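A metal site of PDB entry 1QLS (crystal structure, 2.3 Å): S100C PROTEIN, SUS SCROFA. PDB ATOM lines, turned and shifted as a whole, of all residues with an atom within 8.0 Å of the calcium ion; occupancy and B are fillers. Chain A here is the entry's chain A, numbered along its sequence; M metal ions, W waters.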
ATOM      1  N   PHE A  19     -16.403 -27.144 -21.449  1.00  0.00           N
ATOM      2  CA  PHE A  19     -15.965 -26.062 -20.561  1.00  0.00           C
ATOM      3  C   PHE A  19     -14.455 -25.874 -20.627  1.00  0.00           C
ATOM      4  O   PHE A  19     -13.943 -24.762 -20.778  1.00  0.00           O
ATOM      5  CB  PHE A  19     -16.341 -26.358 -19.125  1.00  0.00           C
ATOM      6  CG  PHE A  19     -15.859 -25.338 -18.167  1.00  0.00           C
ATOM      7  CD1 PHE A  19     -16.582 -24.156 -17.987  1.00  0.00           C
ATOM      8  CD2 PHE A  19     -14.676 -25.531 -17.415  1.00  0.00           C
ATOM      9  CE1 PHE A  19     -16.182 -23.192 -17.118  1.00  0.00           C
ATOM     10  CE2 PHE A  19     -14.265 -24.561 -16.534  1.00  0.00           C
ATOM     11  CZ  PHE A  19     -14.998 -23.385 -16.365  1.00  0.00           C
ATOM     12  N   GLN A  20     -13.728 -26.951 -20.539  1.00  0.00           N
ATOM     13  CA  GLN A  20     -12.271 -26.954 -20.504  1.00  0.00           C
ATOM     14  C   GLN A  20     -11.613 -26.443 -21.741  1.00  0.00           C
ATOM     15  O   GLN A  20     -10.653 -25.637 -21.735  1.00  0.00           O
ATOM     16  CB  GLN A  20     -11.789 -28.356 -20.048  1.00  0.00           C
ATOM     17  CG  GLN A  20     -11.027 -28.231 -18.723  1.00  0.00           C
ATOM     18  CD  GLN A  20     -11.729 -27.796 -17.483  1.00  0.00           C
ATOM     19  OE1 GLN A  20     -12.890 -28.170 -17.198  1.00  0.00           O
ATOM     20  NE2 GLN A  20     -11.114 -26.995 -16.632  1.00  0.00           N
ATOM     21  N   LYS A  21     -12.159 -26.787 -22.894  1.00  0.00           N
ATOM     22  CA  LYS A  21     -11.691 -26.266 -24.164  1.00  0.00           C
ATOM     23  C   LYS A  21     -11.903 -24.735 -24.228  1.00  0.00           C
ATOM     24  O   LYS A  21     -11.004 -24.017 -24.710  1.00  0.00           O
ATOM     25  CB  LYS A  21     -12.544 -26.824 -25.298  1.00  0.00           C
ATOM     26  CG  LYS A  21     -12.030 -26.275 -26.660  1.00  0.00           C
ATOM     27  CD  LYS A  21     -12.878 -26.903 -27.744  1.00  0.00           C
ATOM     28  CE  LYS A  21     -12.851 -26.131 -29.057  1.00  0.00           C
ATOM     29  NZ  LYS A  21     -14.012 -26.560 -29.916  1.00  0.00           N
ATOM     30  N   HIS A  22     -13.063 -24.267 -23.792  1.00  0.00           N
ATOM     31  CA  HIS A  22     -13.302 -22.818 -23.871  1.00  0.00           C
ATOM     32  C   HIS A  22     -12.655 -22.078 -22.729  1.00  0.00           C
ATOM     33  O   HIS A  22     -12.220 -20.938 -22.875  1.00  0.00           O
ATOM     34  CB  HIS A  22     -14.811 -22.494 -23.930  1.00  0.00           C
ATOM     35  CG  HIS A  22     -15.276 -22.938 -25.314  1.00  0.00           C
ATOM     36  ND1 HIS A  22     -15.736 -24.236 -25.533  1.00  0.00           N
ATOM     37  CD2 HIS A  22     -15.310 -22.288 -26.488  1.00  0.00           C
ATOM     38  CE1 HIS A  22     -16.055 -24.364 -26.809  1.00  0.00           C
ATOM     39  NE2 HIS A  22     -15.811 -23.195 -27.404  1.00  0.00           N
ATOM     40  N   ALA A  23     -12.530 -22.773 -21.557  1.00  0.00           N
ATOM     41  CA  ALA A  23     -11.876 -22.056 -20.460  1.00  0.00           C
ATOM     42  C   ALA A  23     -10.382 -22.098 -20.675  1.00  0.00           C
ATOM     43  O   ALA A  23      -9.716 -21.260 -20.085  1.00  0.00           O
ATOM     44  CB  ALA A  23     -12.132 -22.689 -19.105  1.00  0.00           C
ATOM     45  N   GLY A  24      -9.750 -22.976 -21.409  1.00  0.00           N
ATOM     46  CA  GLY A  24      -8.310 -23.001 -21.516  1.00  0.00           C
ATOM     47  C   GLY A  24      -7.697 -22.172 -22.596  1.00  0.00           C
ATOM     48  O   GLY A  24      -6.558 -22.487 -22.919  1.00  0.00           O
ATOM     49  N   ARG A  25      -8.313 -21.074 -23.077  1.00  0.00           N
ATOM     50  CA  ARG A  25      -7.638 -20.299 -24.100  1.00  0.00           C
ATOM     51  C   ARG A  25      -6.655 -19.336 -23.414  1.00  0.00           C
ATOM     52  O   ARG A  25      -5.655 -19.025 -24.023  1.00  0.00           O
ATOM     53  CB  ARG A  25      -8.581 -19.387 -24.913  1.00  0.00           C
ATOM     54  CG  ARG A  25      -9.842 -19.928 -25.478  1.00  0.00           C
ATOM     55  CD  ARG A  25      -9.653 -21.184 -26.327  1.00  0.00           C
ATOM     56  NE  ARG A  25     -10.983 -21.468 -26.940  1.00  0.00           N
ATOM     57  CZ  ARG A  25     -11.347 -21.189 -28.183  1.00  0.00           C
ATOM     58  NH1 ARG A  25     -10.540 -20.604 -29.057  1.00  0.00           N
ATOM     59  NH2 ARG A  25     -12.572 -21.505 -28.539  1.00  0.00           N
ATOM     60  N   ASP A  26      -6.976 -18.801 -22.240  1.00  0.00           N
ATOM     61  CA  ASP A  26      -6.011 -17.901 -21.630  1.00  0.00           C
ATOM     62  C   ASP A  26      -5.220 -18.719 -20.567  1.00  0.00           C
ATOM     63  O   ASP A  26      -5.203 -19.967 -20.636  1.00  0.00           O
ATOM     64  CB  ASP A  26      -6.659 -16.644 -21.111  1.00  0.00           C
ATOM     65  CG  ASP A  26      -7.643 -16.847 -20.018  1.00  0.00           C
ATOM     66  OD1 ASP A  26      -7.677 -18.044 -19.585  1.00  0.00           O
ATOM     67  OD2 ASP A  26      -8.399 -16.044 -19.449  1.00  0.00           O
ATOM     68  N   GLY A  27      -4.572 -18.075 -19.585  1.00  0.00           N
ATOM     69  CA  GLY A  27      -3.794 -18.857 -18.614  1.00  0.00           C
ATOM     70  C   GLY A  27      -4.525 -19.442 -17.438  1.00  0.00           C
ATOM     71  O   GLY A  27      -3.902 -19.945 -16.508  1.00  0.00           O
ATOM     72  N   ASN A  28      -5.868 -19.304 -17.414  1.00  0.00           N
ATOM     73  CA  ASN A  28      -6.633 -19.855 -16.311  1.00  0.00           C
ATOM     74  C   ASN A  28      -7.589 -20.884 -16.792  1.00  0.00           C
ATOM     75  O   ASN A  28      -8.710 -20.533 -17.079  1.00  0.00           O
ATOM     76  CB  ASN A  28      -7.325 -18.727 -15.554  1.00  0.00           C
ATOM     77  CG  ASN A  28      -8.089 -19.170 -14.349  1.00  0.00           C
ATOM     78  OD1 ASN A  28      -8.233 -20.356 -14.049  1.00  0.00           O
ATOM     79  ND2 ASN A  28      -8.588 -18.195 -13.612  1.00  0.00           N
ATOM     80  N   ASN A  29      -7.377 -22.194 -16.829  1.00  0.00           N
ATOM     81  CA  ASN A  29      -8.458 -23.057 -17.352  1.00  0.00           C
ATOM     82  C   ASN A  29      -9.501 -23.401 -16.383  1.00  0.00           C
ATOM     83  O   ASN A  29     -10.223 -24.393 -16.660  1.00  0.00           O
ATOM     84  CB  ASN A  29      -7.828 -24.315 -17.940  1.00  0.00           C
ATOM     85  CG  ASN A  29      -7.087 -25.085 -16.813  1.00  0.00           C
ATOM     86  OD1 ASN A  29      -6.391 -26.029 -17.191  1.00  0.00           O
ATOM     87  ND2 ASN A  29      -7.156 -24.748 -15.571  1.00  0.00           N
ATOM     88  N   THR A  30      -9.721 -22.696 -15.293  1.00  0.00           N
ATOM     89  CA  THR A  30     -10.809 -23.075 -14.414  1.00  0.00           C
ATOM     90  C   THR A  30     -11.874 -21.989 -14.483  1.00  0.00           C
ATOM     91  O   THR A  30     -12.910 -22.066 -13.807  1.00  0.00           O
ATOM     92  CB  THR A  30     -10.354 -23.196 -12.910  1.00  0.00           C
ATOM     93  OG1 THR A  30     -10.021 -21.876 -12.484  1.00  0.00           O
ATOM     94  CG2 THR A  30      -9.107 -24.085 -12.778  1.00  0.00           C
ATOM     95  N   LYS A  31     -11.630 -20.977 -15.346  1.00  0.00           N
ATOM     96  CA  LYS A  31     -12.657 -19.882 -15.395  1.00  0.00           C
ATOM     97  C   LYS A  31     -12.981 -19.464 -16.809  1.00  0.00           C
ATOM     98  O   LYS A  31     -12.066 -19.515 -17.651  1.00  0.00           O
ATOM     99  CB  LYS A  31     -12.073 -18.678 -14.580  1.00  0.00           C
ATOM    100  CG  LYS A  31     -12.702 -18.791 -13.154  1.00  0.00           C
ATOM    101  CD  LYS A  31     -12.227 -17.618 -12.341  1.00  0.00           C
ATOM    102  CE  LYS A  31     -12.540 -17.842 -10.833  1.00  0.00           C
ATOM    103  NZ  LYS A  31     -13.104 -19.212 -10.698  1.00  0.00           N
ATOM    104  N   ILE A  32     -14.211 -19.200 -17.236  1.00  0.00           N
ATOM    105  CA  ILE A  32     -14.340 -18.744 -18.648  1.00  0.00           C
ATOM    106  C   ILE A  32     -14.327 -17.250 -18.586  1.00  0.00           C
ATOM    107  O   ILE A  32     -15.175 -16.661 -17.827  1.00  0.00           O
ATOM    108  CB  ILE A  32     -15.670 -19.330 -19.218  1.00  0.00           C
ATOM    109  CG1 ILE A  32     -15.375 -20.729 -19.757  1.00  0.00           C
ATOM    110  CG2 ILE A  32     -16.182 -18.472 -20.416  1.00  0.00           C
ATOM    111  CD1 ILE A  32     -16.595 -21.494 -20.231  1.00  0.00           C
ATOM    112  N   SER A  33     -13.352 -16.536 -19.204  1.00  0.00           N
ATOM    113  CA  SER A  33     -13.525 -15.052 -19.059  1.00  0.00           C
ATOM    114  C   SER A  33     -14.622 -14.518 -20.067  1.00  0.00           C
ATOM    115  O   SER A  33     -15.222 -15.272 -20.856  1.00  0.00           O
ATOM    116  CB  SER A  33     -12.190 -14.424 -19.497  1.00  0.00           C
ATOM    117  OG  SER A  33     -12.042 -14.683 -20.904  1.00  0.00           O
ATOM    118  N   LYS A  34     -14.881 -13.241 -20.061  1.00  0.00           N
ATOM    119  CA  LYS A  34     -15.838 -12.554 -20.951  1.00  0.00           C
ATOM    120  C   LYS A  34     -15.471 -12.802 -22.407  1.00  0.00           C
ATOM    121  O   LYS A  34     -16.277 -13.265 -23.188  1.00  0.00           O
ATOM    122  CB  LYS A  34     -15.790 -11.050 -20.709  1.00  0.00           C
ATOM    123  CG  LYS A  34     -16.573 -10.272 -21.767  1.00  0.00           C
ATOM    124  CD  LYS A  34     -17.913  -9.802 -21.190  1.00  0.00           C
ATOM    125  CE  LYS A  34     -17.873  -8.280 -21.026  1.00  0.00           C
ATOM    126  NZ  LYS A  34     -19.222  -7.744 -20.636  1.00  0.00           N
ATOM    127  N   GLU A  36     -13.740 -15.339 -23.649  1.00  0.00           N
ATOM    128  CA  GLU A  36     -13.956 -16.734 -23.922  1.00  0.00           C
ATOM    129  C   GLU A  36     -15.448 -17.046 -23.941  1.00  0.00           C
ATOM    130  O   GLU A  36     -15.756 -17.977 -24.650  1.00  0.00           O
ATOM    131  CB  GLU A  36     -13.366 -17.637 -22.779  1.00  0.00           C
ATOM    132  CG  GLU A  36     -11.865 -17.708 -22.959  1.00  0.00           C
ATOM    133  CD  GLU A  36     -11.149 -18.130 -21.652  1.00  0.00           C
ATOM    134  OE1 GLU A  36     -11.752 -18.061 -20.567  1.00  0.00           O
ATOM    135  OE2 GLU A  36      -9.974 -18.494 -21.728  1.00  0.00           O
ATOM    136  N   GLN A  72     -15.986 -13.688 -14.213  1.00  0.00           N
ATOM    137  CA  GLN A  72     -15.605 -14.831 -15.088  1.00  0.00           C
ATOM    138  C   GLN A  72     -16.588 -15.949 -14.913  1.00  0.00           C
ATOM    139  O   GLN A  72     -17.343 -15.773 -13.966  1.00  0.00           O
ATOM    140  CB  GLN A  72     -14.198 -15.325 -14.683  1.00  0.00           C
ATOM    141  CG  GLN A  72     -13.131 -14.278 -15.083  1.00  0.00           C
ATOM    142  CD  GLN A  72     -11.813 -14.911 -15.341  1.00  0.00           C
ATOM    143  OE1 GLN A  72     -11.670 -15.571 -16.375  1.00  0.00           O
ATOM    144  NE2 GLN A  72     -10.845 -14.728 -14.439  1.00  0.00           N
ATOM    145  N   LEU A  73     -16.762 -17.014 -15.649  1.00  0.00           N
ATOM    146  CA  LEU A  73     -17.774 -17.993 -15.278  1.00  0.00           C
ATOM    147  C   LEU A  73     -16.954 -19.215 -14.783  1.00  0.00           C
ATOM    148  O   LEU A  73     -16.017 -19.625 -15.485  1.00  0.00           O
ATOM    149  CB  LEU A  73     -18.633 -18.464 -16.461  1.00  0.00           C
ATOM    150  CG  LEU A  73     -19.452 -17.336 -17.168  1.00  0.00           C
ATOM    151  CD1 LEU A  73     -20.341 -17.850 -18.293  1.00  0.00           C
ATOM    152  CD2 LEU A  73     -20.310 -16.589 -16.180  1.00  0.00           C
HETATM  153 CA    CA M   1      -9.924 -19.055 -18.962  1.00  0.00          CA
HETATM  154  O   HOH W   1     -10.033 -16.962 -17.617  1.00  0.00           O
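The backbone NH (N) of Glu 36 is in hydrogen-bond range of the side-chain hydroxyl (OG) of Ser 33 (3.3 Å).
OD1 of Asn 28 is in hydrogen-bond range of OG1 of Thr 30.
OE2 of Glu 36 sits close to N of Arg 25 (3.4 Å).
Water W1 lies within hydrogen-bond range of OE1 of Gln 72 (2.5 Å) and OD2 of Asp 26 (2.6 Å).
The calcium ion is bound by O of Ala 23 (2.5 Å), water W1 (2.5 Å), OD1 of Asp 26 (2.5 Å), O of Lys 31 (2.6 Å), OE1 of Glu 36 (2.6 Å), O of Asn 28 (2.7 Å) and OE2 of Glu 36 (2.8 Å).
The calcium ion has seven donor atoms within binding distance.
Within 4 Å of the calcium ion: Ala 23, Asp 26, Asn 28, Lys 31 and Glu 36.
Along chain A the residues within 4 Å of the calcium ion span positions 23 to 36.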
